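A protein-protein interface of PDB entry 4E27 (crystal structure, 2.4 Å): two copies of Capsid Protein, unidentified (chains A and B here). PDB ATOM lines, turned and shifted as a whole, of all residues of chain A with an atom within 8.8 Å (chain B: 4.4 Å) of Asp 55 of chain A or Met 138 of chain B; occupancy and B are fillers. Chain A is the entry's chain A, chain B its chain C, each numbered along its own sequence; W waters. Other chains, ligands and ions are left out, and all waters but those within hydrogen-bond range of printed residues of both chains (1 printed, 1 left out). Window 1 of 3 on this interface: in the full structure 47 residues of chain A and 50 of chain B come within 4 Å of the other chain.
The backbone carbonyl oxygen of Met 138 of chain B lies within hydrogen-bond range of the backbone NH of Phe 60 of chain A (3.0 Å).
O of Phe 60 of chain A sits at hydrogen-bond distance from N of Lys 140 of chain B, at 2.9 Å.
The side-chain carboxylate (OE2) of Glu 54 of chain B lies within salt-bridge range of the guanidinium group (NE) of Arg 53 of chain A, at 3.7 Å.
The side-chain carboxylate of Asp 55 of chain A is in salt-bridge range of the side-chain amino group of Lys 58 of chain B (3.0 Å).
NE of Arg 53 of chain A is in salt-bridge range of OD1 of Asp 55 of chain A, at 2.7 Å.
The side-chain amide nitrogen (ND2) of Asn 64 of chain A lies within hydrogen-bond range of the backbone carbonyl oxygen (O) of Ala 59 of chain A (3.2 Å).
The backbone carbonyl oxygen of Phe 83 of chain B is in hydrogen-bond range of the backbone NH of Ile 165 of chain B (2.8 Å).
O of Val 87 of chain A lies within hydrogen-bond range of N of Ile 161 of chain A, at 3.0 Å.
The backbone carbonyl oxygen of Ala 59 of chain A lies within hydrogen-bond range of the guanidinium group of Arg 163 of chain A, 2.8 Å away.
N of Thr 61 of chain A lies within hydrogen-bond range of OD1 of Asn 64 of chain A, 2.8 Å away.
Arg 53 of chain A touches Lys 58 of chain B.
Ile 165 of chain B touches Arg 53 of chain A (CG2 to NH2, 3.6 Å).
Asp 55 of chain A touches Glu 54 of chain B (CG to OE1, 3.5 Å).
Leu 56 of chain A touches Ile 165 of chain B (CD2 to CG2, 3.9 Å).
CB of Ala 59 of chain A touches CD2 of Phe 83 of chain B (3.995 Å).
Ala 59 of chain A touches Met 138 of chain B (CA to O, 3.4 Å).
CB of Ala 59 of chain A touches CB of Lys 140 of chain B (3.98 Å).
O of Phe 60 of chain A touches CA of Val 139 of chain B, 3.4 Å away.
Lys 140 of chain B touches Thr 61 of chain A (O to CG2, 3.4 Å).
Pro 175 of chain A touches Phe 83 of chain B.
Of the printed residues of chain B, Arg 53 of chain A touches Glu 54 (3.3 Å), Lys 58 (3.8 Å) and Ile 165 (3.6 Å).
Asp 55 of chain A touches three residues of chain B.
Printed residues of chain B within 4 Å of Leu 56 of chain A: Phe 83 and Ile 165.
Gln 57 of chain A touches none of the printed residues of chain B.
Arg 163 of chain A touches none of the printed residues of chain B.
Printed residues of chain A within 4 Å of Glu 54 of chain B: Arg 53 (3.3 Å) and Asp 55 (3.5 Å).
Printed residues of chain A within 4 Å of Phe 83 of chain B: Leu 56, Ala 59 and Pro 175.
Of the printed residues of chain A, Lys 140 of chain B touches Ala 59 (3.98 Å), Phe 60 (2.9 Å), Thr 61 (3.4 Å) and Pro 175 (3.5 Å).
The nearest residue of chain A that does not touch Met 138 of chain B is Leu 56 of chain A (4.2 Å).
The nearest printed residue of chain B that does not touch Pro 175 of chain A is Val 139 of chain B (7.3 Å).
Of the 10 printed residues of chain B, 8 touch a printed residue of chain A.
Hydrophobic or aromatic side chains of chain B within 4 Å of the printed part of chain A: Phe 83, Leu 137, Met 138, Val 139 and Ile 165.
Along chain B the printed residues that touch a printed residue of chain A span positions 54 to 165.
Printed residues of chain A that touch a printed residue of chain B: Arg 53, Asp 55, Leu 56, Ala 59, Phe 60, Thr 61, Ile 161 and Pro 175.
Hydrophobic or aromatic side chains of chain A that line the printed part of chain B: Leu 56, Ala 59, Ile 161 and Pro 175.
Along chain A the printed residues that touch a printed residue of chain B span positions 53 to 175.
Among the printed residues, Asp or Glu carboxylates within 4 Å of a Lys or Arg side-chain nitrogen of the other chain: Arg 53 of chain A with Glu 54 of chain B (3.7 Å) and Asp 55 of chain A with Lys 58 of chain B (3.0 Å).
Positions printed for both chains: 54, 58, 85 and 165.
Water W1 bridges O of Pro 175 of chain A and NZ of Lys 140 of chain B.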
ATOM      1  N   ALA A  51      17.094 -16.535 -24.797  1.00  0.00           N
ATOM      2  CA  ALA A  51      17.757 -15.262 -25.067  1.00  0.00           C
ATOM      3  C   ALA A  51      17.017 -14.530 -26.176  1.00  0.00           C
ATOM      4  O   ALA A  51      17.608 -14.109 -27.164  1.00  0.00           O
ATOM      5  CB  ALA A  51      19.209 -15.481 -25.440  1.00  0.00           C
ATOM      6  N   GLN A  52      15.708 -14.409 -26.014  1.00  0.00           N
ATOM      7  CA  GLN A  52      14.867 -13.799 -27.027  1.00  0.00           C
ATOM      8  C   GLN A  52      14.654 -12.326 -26.760  1.00  0.00           C
ATOM      9  O   GLN A  52      14.031 -11.634 -27.549  1.00  0.00           O
ATOM     10  CB  GLN A  52      13.507 -14.496 -27.072  1.00  0.00           C
ATOM     11  CG  GLN A  52      13.573 -15.877 -27.658  1.00  0.00           C
ATOM     12  CD  GLN A  52      14.216 -15.878 -29.024  1.00  0.00           C
ATOM     13  OE1 GLN A  52      13.843 -15.097 -29.894  1.00  0.00           O
ATOM     14  NE2 GLN A  52      15.181 -16.770 -29.227  1.00  0.00           N
ATOM     15  N   ARG A  53      15.142 -11.852 -25.626  1.00  0.00           N
ATOM     16  CA  ARG A  53      15.010 -10.448 -25.297  1.00  0.00           C
ATOM     17  C   ARG A  53      16.392  -9.819 -25.297  1.00  0.00           C
ATOM     18  O   ARG A  53      17.363 -10.472 -24.931  1.00  0.00           O
ATOM     19  CB  ARG A  53      14.323 -10.280 -23.944  1.00  0.00           C
ATOM     20  CG  ARG A  53      13.731  -8.904 -23.711  1.00  0.00           C
ATOM     21  CD  ARG A  53      12.968  -8.882 -22.388  1.00  0.00           C
ATOM     22  NE  ARG A  53      13.855  -9.112 -21.257  1.00  0.00           N
ATOM     23  CZ  ARG A  53      13.444  -9.399 -20.024  1.00  0.00           C
ATOM     24  NH1 ARG A  53      12.144  -9.498 -19.757  1.00  0.00           N
ATOM     25  NH2 ARG A  53      14.336  -9.581 -19.055  1.00  0.00           N
ATOM     26  N   GLU A  54      16.463  -8.555 -25.714  1.00  0.00           N
ATOM     27  CA  GLU A  54      17.722  -7.841 -25.916  1.00  0.00           C
ATOM     28  C   GLU A  54      18.700  -7.993 -24.747  1.00  0.00           C
ATOM     29  O   GLU A  54      19.884  -8.269 -24.954  1.00  0.00           O
ATOM     30  CB  GLU A  54      17.448  -6.359 -26.227  1.00  0.00           C
ATOM     31  CG  GLU A  54      18.682  -5.496 -26.501  1.00  0.00           C
ATOM     32  CD  GLU A  54      18.341  -4.145 -27.141  1.00  0.00           C
ATOM     33  OE1 GLU A  54      19.166  -3.211 -27.044  1.00  0.00           O
ATOM     34  OE2 GLU A  54      17.259  -4.014 -27.755  1.00  0.00           O
ATOM     35  N   ASP A  55      18.202  -7.861 -23.524  1.00  0.00           N
ATOM     36  CA  ASP A  55      19.070  -7.869 -22.352  1.00  0.00           C
ATOM     37  C   ASP A  55      19.676  -9.241 -22.066  1.00  0.00           C
ATOM     38  O   ASP A  55      20.801  -9.331 -21.578  1.00  0.00           O
ATOM     39  CB  ASP A  55      18.333  -7.346 -21.117  1.00  0.00           C
ATOM     40  CG  ASP A  55      17.150  -8.224 -20.729  1.00  0.00           C
ATOM     41  OD1 ASP A  55      16.551  -8.866 -21.626  1.00  0.00           O
ATOM     42  OD2 ASP A  55      16.829  -8.272 -19.523  1.00  0.00           O
ATOM     43  N   LEU A  56      18.937 -10.304 -22.358  1.00  0.00           N
ATOM     44  CA  LEU A  56      19.450 -11.663 -22.171  1.00  0.00           C
ATOM     45  C   LEU A  56      20.444 -12.035 -23.292  1.00  0.00           C
ATOM     46  O   LEU A  56      21.493 -12.649 -23.052  1.00  0.00           O
ATOM     47  CB  LEU A  56      18.300 -12.680 -22.138  1.00  0.00           C
ATOM     48  CG  LEU A  56      17.118 -12.478 -21.169  1.00  0.00           C
ATOM     49  CD1 LEU A  56      16.138 -13.599 -21.310  1.00  0.00           C
ATOM     50  CD2 LEU A  56      17.585 -12.373 -19.720  1.00  0.00           C
ATOM     51  N   GLN A  57      20.106 -11.658 -24.520  1.00  0.00           N
ATOM     52  CA  GLN A  57      20.947 -11.961 -25.662  1.00  0.00           C
ATOM     53  C   GLN A  57      22.334 -11.312 -25.557  1.00  0.00           C
ATOM     54  O   GLN A  57      23.303 -11.844 -26.102  1.00  0.00           O
ATOM     55  CB  GLN A  57      20.238 -11.561 -26.966  1.00  0.00           C
ATOM     56  CG  GLN A  57      20.991 -11.901 -28.230  1.00  0.00           C
ATOM     57  CD  GLN A  57      21.966 -10.814 -28.615  1.00  0.00           C
ATOM     58  OE1 GLN A  57      21.700  -9.634 -28.388  1.00  0.00           O
ATOM     59  NE2 GLN A  57      23.108 -11.200 -29.187  1.00  0.00           N
ATOM     60  N   LYS A  58      22.431 -10.173 -24.865  1.00  0.00           N
ATOM     61  CA  LYS A  58      23.710  -9.443 -24.778  1.00  0.00           C
ATOM     62  C   LYS A  58      24.526  -9.800 -23.536  1.00  0.00           C
ATOM     63  O   LYS A  58      25.548  -9.162 -23.259  1.00  0.00           O
ATOM     64  CB  LYS A  58      23.497  -7.927 -24.826  1.00  0.00           C
ATOM     65  CG  LYS A  58      22.828  -7.439 -26.107  1.00  0.00           C
ATOM     66  CD  LYS A  58      22.344  -5.986 -25.997  1.00  0.00           C
ATOM     67  CE  LYS A  58      23.512  -5.028 -26.048  1.00  0.00           C
ATOM     68  NZ  LYS A  58      23.059  -3.635 -26.350  1.00  0.00           N
ATOM     69  N   ALA A  59      24.065 -10.810 -22.801  1.00  0.00           N
ATOM     70  CA  ALA A  59      24.719 -11.253 -21.567  1.00  0.00           C
ATOM     71  C   ALA A  59      26.201 -11.592 -21.718  1.00  0.00           C
ATOM     72  O   ALA A  59      26.652 -12.097 -22.753  1.00  0.00           O
ATOM     73  CB  ALA A  59      23.990 -12.451 -20.977  1.00  0.00           C
ATOM     74  N   PHE A  60      26.951 -11.322 -20.659  1.00  0.00           N
ATOM     75  CA  PHE A  60      28.335 -11.754 -20.588  1.00  0.00           C
ATOM     76  C   PHE A  60      28.409 -13.159 -20.018  1.00  0.00           C
ATOM     77  O   PHE A  60      27.682 -13.508 -19.090  1.00  0.00           O
ATOM     78  CB  PHE A  60      29.146 -10.778 -19.739  1.00  0.00           C
ATOM     79  CG  PHE A  60      29.400  -9.464 -20.420  1.00  0.00           C
ATOM     80  CD1 PHE A  60      30.387  -9.354 -21.382  1.00  0.00           C
ATOM     81  CD2 PHE A  60      28.631  -8.347 -20.121  1.00  0.00           C
ATOM     82  CE1 PHE A  60      30.611  -8.156 -22.028  1.00  0.00           C
ATOM     83  CE2 PHE A  60      28.862  -7.137 -20.762  1.00  0.00           C
ATOM     84  CZ  PHE A  60      29.846  -7.047 -21.717  1.00  0.00           C
ATOM     85  N   THR A  61      29.273 -13.977 -20.600  1.00  0.00           N
ATOM     86  CA  THR A  61      29.549 -15.296 -20.058  1.00  0.00           C
ATOM     87  C   THR A  61      31.048 -15.417 -19.890  1.00  0.00           C
ATOM     88  O   THR A  61      31.799 -14.633 -20.457  1.00  0.00           O
ATOM     89  CB  THR A  61      29.067 -16.420 -21.002  1.00  0.00           C
ATOM     90  OG1 THR A  61      29.817 -16.380 -22.226  1.00  0.00           O
ATOM     91  CG2 THR A  61      27.580 -16.269 -21.307  1.00  0.00           C
ATOM     92  N   LEU A  62      31.474 -16.400 -19.107  1.00  0.00           N
ATOM     93  CA  LEU A  62      32.884 -16.708 -18.935  1.00  0.00           C
ATOM     94  C   LEU A  62      33.592 -16.965 -20.274  1.00  0.00           C
ATOM     95  O   LEU A  62      34.751 -16.602 -20.465  1.00  0.00           O
ATOM     96  CB  LEU A  62      33.017 -17.938 -18.044  1.00  0.00           C
ATOM     97  CG  LEU A  62      34.428 -18.438 -17.784  1.00  0.00           C
ATOM     98  CD1 LEU A  62      35.278 -17.314 -17.204  1.00  0.00           C
ATOM     99  CD2 LEU A  62      34.339 -19.607 -16.835  1.00  0.00           C
ATOM    100  N   ASN A  64      32.505 -15.845 -23.439  1.00  0.00           N
ATOM    101  CA  ASN A  64      32.416 -14.815 -24.471  1.00  0.00           C
ATOM    102  C   ASN A  64      33.044 -13.491 -24.057  1.00  0.00           C
ATOM    103  O   ASN A  64      33.270 -12.597 -24.877  1.00  0.00           O
ATOM    104  CB  ASN A  64      30.977 -14.635 -24.991  1.00  0.00           C
ATOM    105  CG  ASN A  64      30.059 -13.881 -24.017  1.00  0.00           C
ATOM    106  OD1 ASN A  64      30.496 -13.280 -23.031  1.00  0.00           O
ATOM    107  ND2 ASN A  64      28.764 -13.910 -24.312  1.00  0.00           N
ATOM    108  N   THR A  65      33.337 -13.390 -22.773  1.00  0.00           N
ATOM    109  CA  THR A  65      33.837 -12.155 -22.219  1.00  0.00           C
ATOM    110  C   THR A  65      35.279 -11.916 -22.641  1.00  0.00           C
ATOM    111  O   THR A  65      36.143 -12.771 -22.453  1.00  0.00           O
ATOM    112  CB  THR A  65      33.672 -12.150 -20.685  1.00  0.00           C
ATOM    113  OG1 THR A  65      32.273 -12.116 -20.381  1.00  0.00           O
ATOM    114  CG2 THR A  65      34.373 -10.954 -20.036  1.00  0.00           C
ATOM    115  N   LYS A  85      29.995  -4.976 -27.911  1.00  0.00           N
ATOM    116  CA  LYS A  85      29.638  -4.181 -26.758  1.00  0.00           C
ATOM    117  C   LYS A  85      30.907  -4.075 -25.937  1.00  0.00           C
ATOM    118  O   LYS A  85      31.555  -5.077 -25.688  1.00  0.00           O
ATOM    119  CB  LYS A  85      28.541  -4.873 -25.959  1.00  0.00           C
ATOM    120  CG  LYS A  85      28.453  -4.393 -24.534  1.00  0.00           C
ATOM    121  CD  LYS A  85      27.159  -4.814 -23.860  1.00  0.00           C
ATOM    122  CE  LYS A  85      26.962  -4.022 -22.567  1.00  0.00           C
ATOM    123  NZ  LYS A  85      25.737  -4.413 -21.815  1.00  0.00           N
ATOM    124  N   VAL A  87      32.311  -2.081 -22.332  1.00  0.00           N
ATOM    125  CA  VAL A  87      32.023  -1.209 -21.181  1.00  0.00           C
ATOM    126  C   VAL A  87      33.176  -1.239 -20.190  1.00  0.00           C
ATOM    127  O   VAL A  87      33.941  -2.199 -20.167  1.00  0.00           O
ATOM    128  CB  VAL A  87      30.731  -1.637 -20.440  1.00  0.00           C
ATOM    129  CG1 VAL A  87      29.554  -1.681 -21.398  1.00  0.00           C
ATOM    130  CG2 VAL A  87      30.913  -2.989 -19.789  1.00  0.00           C
ATOM    131  N   ILE A 161      35.317  -4.849 -20.157  1.00  0.00           N
ATOM    132  CA  ILE A 161      34.941  -6.128 -20.727  1.00  0.00           C
ATOM    133  C   ILE A 161      34.273  -5.839 -22.046  1.00  0.00           C
ATOM    134  O   ILE A 161      33.656  -4.790 -22.224  1.00  0.00           O
ATOM    135  CB  ILE A 161      33.942  -6.908 -19.829  1.00  0.00           C
ATOM    136  CG1 ILE A 161      32.698  -6.066 -19.561  1.00  0.00           C
ATOM    137  CG2 ILE A 161      34.596  -7.332 -18.513  1.00  0.00           C
ATOM    138  CD1 ILE A 161      31.671  -6.736 -18.644  1.00  0.00           C
ATOM    139  N   ARG A 163      32.290  -8.006 -25.671  1.00  0.00           N
ATOM    140  CA  ARG A 163      31.882  -9.251 -26.307  1.00  0.00           C
ATOM    141  C   ARG A 163      31.256  -8.979 -27.660  1.00  0.00           C
ATOM    142  O   ARG A 163      30.793  -7.868 -27.937  1.00  0.00           O
ATOM    143  CB  ARG A 163      30.931 -10.074 -25.430  1.00  0.00           C
ATOM    144  CG  ARG A 163      29.551  -9.465 -25.210  1.00  0.00           C
ATOM    145  CD  ARG A 163      28.493 -10.547 -25.010  1.00  0.00           C
ATOM    146  NE  ARG A 163      28.106 -11.158 -26.282  1.00  0.00           N
ATOM    147  CZ  ARG A 163      26.968 -11.821 -26.474  1.00  0.00           C
ATOM    148  NH1 ARG A 163      26.107 -11.953 -25.471  1.00  0.00           N
ATOM    149  NH2 ARG A 163      26.681 -12.328 -27.670  1.00  0.00           N
ATOM    150  N   ILE A 165      28.346  -9.061 -30.046  1.00  0.00           N
ATOM    151  CA  ILE A 165      26.887  -9.114 -30.005  1.00  0.00           C
ATOM    152  C   ILE A 165      26.293  -9.674 -31.303  1.00  0.00           C
ATOM    153  O   ILE A 165      25.267 -10.346 -31.283  1.00  0.00           O
ATOM    154  CB  ILE A 165      26.298  -7.716 -29.747  1.00  0.00           C
ATOM    155  CG1 ILE A 165      26.888  -7.125 -28.454  1.00  0.00           C
ATOM    156  CG2 ILE A 165      24.769  -7.769 -29.691  1.00  0.00           C
ATOM    157  CD1 ILE A 165      26.584  -7.939 -27.189  1.00  0.00           C
ATOM    158  N   PRO A 175      24.385 -15.801 -26.200  1.00  0.00           N
ATOM    159  CA  PRO A 175      25.367 -15.714 -25.110  1.00  0.00           C
ATOM    160  C   PRO A 175      25.868 -17.085 -24.647  1.00  0.00           C
ATOM    161  O   PRO A 175      25.217 -18.098 -24.916  1.00  0.00           O
ATOM    162  CB  PRO A 175      24.584 -15.027 -23.986  1.00  0.00           C
ATOM    163  CG  PRO A 175      23.153 -15.327 -24.277  1.00  0.00           C
ATOM    164  CD  PRO A 175      23.032 -15.390 -25.775  1.00  0.00           C
ATOM    165  N   GLU B  54       9.662  -5.556 -19.458  1.00  0.00           N
ATOM    166  CA  GLU B  54      11.036  -5.785 -19.009  1.00  0.00           C
ATOM    167  C   GLU B  54      11.250  -5.238 -17.598  1.00  0.00           C
ATOM    168  O   GLU B  54      11.681  -5.962 -16.713  1.00  0.00           O
ATOM    169  CB  GLU B  54      12.015  -5.149 -20.016  1.00  0.00           C
ATOM    170  CG  GLU B  54      13.427  -5.755 -20.108  1.00  0.00           C
ATOM    171  CD  GLU B  54      14.059  -5.578 -21.511  1.00  0.00           C
ATOM    172  OE1 GLU B  54      15.291  -5.377 -21.625  1.00  0.00           O
ATOM    173  OE2 GLU B  54      13.311  -5.646 -22.512  1.00  0.00           O
ATOM    174  N   LYS B  58      11.813  -7.682 -14.259  1.00  0.00           N
ATOM    175  CA  LYS B  58      13.159  -7.677 -13.669  1.00  0.00           C
ATOM    176  C   LYS B  58      13.202  -7.127 -12.248  1.00  0.00           C
ATOM    177  O   LYS B  58      14.291  -6.940 -11.691  1.00  0.00           O
ATOM    178  CB  LYS B  58      14.146  -6.884 -14.539  1.00  0.00           C
ATOM    179  CG  LYS B  58      14.298  -7.415 -15.958  1.00  0.00           C
ATOM    180  CD  LYS B  58      15.207  -6.518 -16.800  1.00  0.00           C
ATOM    181  CE  LYS B  58      16.632  -6.993 -16.708  1.00  0.00           C
ATOM    182  NZ  LYS B  58      17.532  -6.155 -17.521  1.00  0.00           N
ATOM    183  N   PHE B  83      20.405 -16.746 -16.131  1.00  0.00           N
ATOM    184  CA  PHE B  83      20.846 -15.379 -16.423  1.00  0.00           C
ATOM    185  C   PHE B  83      20.631 -14.554 -15.183  1.00  0.00           C
ATOM    186  O   PHE B  83      19.548 -14.602 -14.599  1.00  0.00           O
ATOM    187  CB  PHE B  83      20.013 -14.728 -17.526  1.00  0.00           C
ATOM    188  CG  PHE B  83      20.174 -15.343 -18.882  1.00  0.00           C
ATOM    189  CD1 PHE B  83      19.601 -16.579 -19.176  1.00  0.00           C
ATOM    190  CD2 PHE B  83      20.840 -14.656 -19.892  1.00  0.00           C
ATOM    191  CE1 PHE B  83      19.725 -17.128 -20.445  1.00  0.00           C
ATOM    192  CE2 PHE B  83      20.965 -15.203 -21.160  1.00  0.00           C
ATOM    193  CZ  PHE B  83      20.410 -16.434 -21.437  1.00  0.00           C
ATOM    194  N   TYR B  84      21.632 -13.776 -14.792  1.00  0.00           N
ATOM    195  CA  TYR B  84      21.524 -12.976 -13.572  1.00  0.00           C
ATOM    196  C   TYR B  84      21.756 -11.499 -13.837  1.00  0.00           C
ATOM    197  O   TYR B  84      22.582 -11.114 -14.667  1.00  0.00           O
ATOM    198  CB  TYR B  84      22.509 -13.475 -12.506  1.00  0.00           C
ATOM    199  CG  TYR B  84      22.280 -14.924 -12.135  1.00  0.00           C
ATOM    200  CD1 TYR B  84      22.785 -15.944 -12.916  1.00  0.00           C
ATOM    201  CD2 TYR B  84      21.536 -15.263 -11.016  1.00  0.00           C
ATOM    202  CE1 TYR B  84      22.569 -17.255 -12.587  1.00  0.00           C
ATOM    203  CE2 TYR B  84      21.312 -16.566 -10.684  1.00  0.00           C
ATOM    204  CZ  TYR B  84      21.827 -17.558 -11.471  1.00  0.00           C
ATOM    205  OH  TYR B  84      21.606 -18.866 -11.135  1.00  0.00           O
ATOM    206  N   LYS B  85      21.016 -10.667 -13.125  1.00  0.00           N
ATOM    207  CA  LYS B  85      21.285  -9.250 -13.144  1.00  0.00           C
ATOM    208  C   LYS B  85      22.039  -8.938 -11.869  1.00  0.00           C
ATOM    209  O   LYS B  85      21.595  -9.318 -10.799  1.00  0.00           O
ATOM    210  CB  LYS B  85      19.982  -8.471 -13.181  1.00  0.00           C
ATOM    211  CG  LYS B  85      20.177  -6.983 -13.089  1.00  0.00           C
ATOM    212  CD  LYS B  85      18.864  -6.249 -12.909  1.00  0.00           C
ATOM    213  CE  LYS B  85      19.102  -4.760 -12.902  1.00  0.00           C
ATOM    214  NZ  LYS B  85      17.825  -4.000 -12.955  1.00  0.00           N
ATOM    215  N   LEU B 137      25.339  -5.337 -14.511  1.00  0.00           N
ATOM    216  CA  LEU B 137      25.665  -6.415 -15.429  1.00  0.00           C
ATOM    217  C   LEU B 137      24.538  -7.424 -15.645  1.00  0.00           C
ATOM    218  O   LEU B 137      23.747  -7.706 -14.733  1.00  0.00           O
ATOM    219  CB  LEU B 137      26.902  -7.157 -14.934  1.00  0.00           C
ATOM    220  CG  LEU B 137      28.226  -6.398 -14.887  1.00  0.00           C
ATOM    221  CD1 LEU B 137      29.128  -6.943 -13.769  1.00  0.00           C
ATOM    222  CD2 LEU B 137      28.929  -6.502 -16.227  1.00  0.00           C
ATOM    223  N   MET B 138      24.482  -7.969 -16.856  1.00  0.00           N
ATOM    224  CA  MET B 138      23.667  -9.140 -17.131  1.00  0.00           C
ATOM    225  C   MET B 138      24.620 -10.294 -17.439  1.00  0.00           C
ATOM    226  O   MET B 138      25.391 -10.236 -18.402  1.00  0.00           O
ATOM    227  CB  MET B 138      22.721  -8.904 -18.301  1.00  0.00           C
ATOM    228  CG  MET B 138      21.872 -10.128 -18.619  1.00  0.00           C
ATOM    229  SD  MET B 138      20.717 -10.588 -17.282  1.00  0.00           S
ATOM    230  CE  MET B 138      19.431  -9.351 -17.511  1.00  0.00           C
ATOM    231  N   VAL B 139      24.593 -11.324 -16.599  1.00  0.00           N
ATOM    232  CA  VAL B 139      25.543 -12.417 -16.715  1.00  0.00           C
ATOM    233  C   VAL B 139      24.804 -13.730 -16.849  1.00  0.00           C
ATOM    234  O   VAL B 139      23.813 -13.968 -16.155  1.00  0.00           O
ATOM    235  CB  VAL B 139      26.462 -12.490 -15.495  1.00  0.00           C
ATOM    236  CG1 VAL B 139      27.336 -13.726 -15.557  1.00  0.00           C
ATOM    237  CG2 VAL B 139      27.319 -11.255 -15.421  1.00  0.00           C
ATOM    238  N   LYS B 140      25.282 -14.571 -17.760  1.00  0.00           N
ATOM    239  CA  LYS B 140      24.710 -15.885 -17.971  1.00  0.00           C
ATOM    240  C   LYS B 140      25.700 -16.954 -17.545  1.00  0.00           C
ATOM    241  O   LYS B 140      26.812 -17.015 -18.073  1.00  0.00           O
ATOM    242  CB  LYS B 140      24.348 -16.102 -19.446  1.00  0.00           C
ATOM    243  CG  LYS B 140      23.941 -17.547 -19.717  1.00  0.00           C
ATOM    244  CD  LYS B 140      23.637 -17.847 -21.177  1.00  0.00           C
ATOM    245  CE  LYS B 140      23.290 -19.338 -21.334  1.00  0.00           C
ATOM    246  NZ  LYS B 140      22.992 -19.703 -22.742  1.00  0.00           N
ATOM    247  N   ILE B 165      17.136 -13.574 -13.498  1.00  0.00           N
ATOM    248  CA  ILE B 165      16.168 -13.032 -14.433  1.00  0.00           C
ATOM    249  C   ILE B 165      15.519 -14.139 -15.269  1.00  0.00           C
ATOM    250  O   ILE B 165      14.340 -14.053 -15.635  1.00  0.00           O
ATOM    251  CB  ILE B 165      16.842 -12.029 -15.389  1.00  0.00           C
ATOM    252  CG1 ILE B 165      17.614 -10.964 -14.598  1.00  0.00           C
ATOM    253  CG2 ILE B 165      15.818 -11.401 -16.340  1.00  0.00           C
ATOM    254  CD1 ILE B 165      16.770 -10.201 -13.566  1.00  0.00           C
HETATM  255  O   HOH W   1      25.938 -19.975 -23.016  1.00  0.00           O
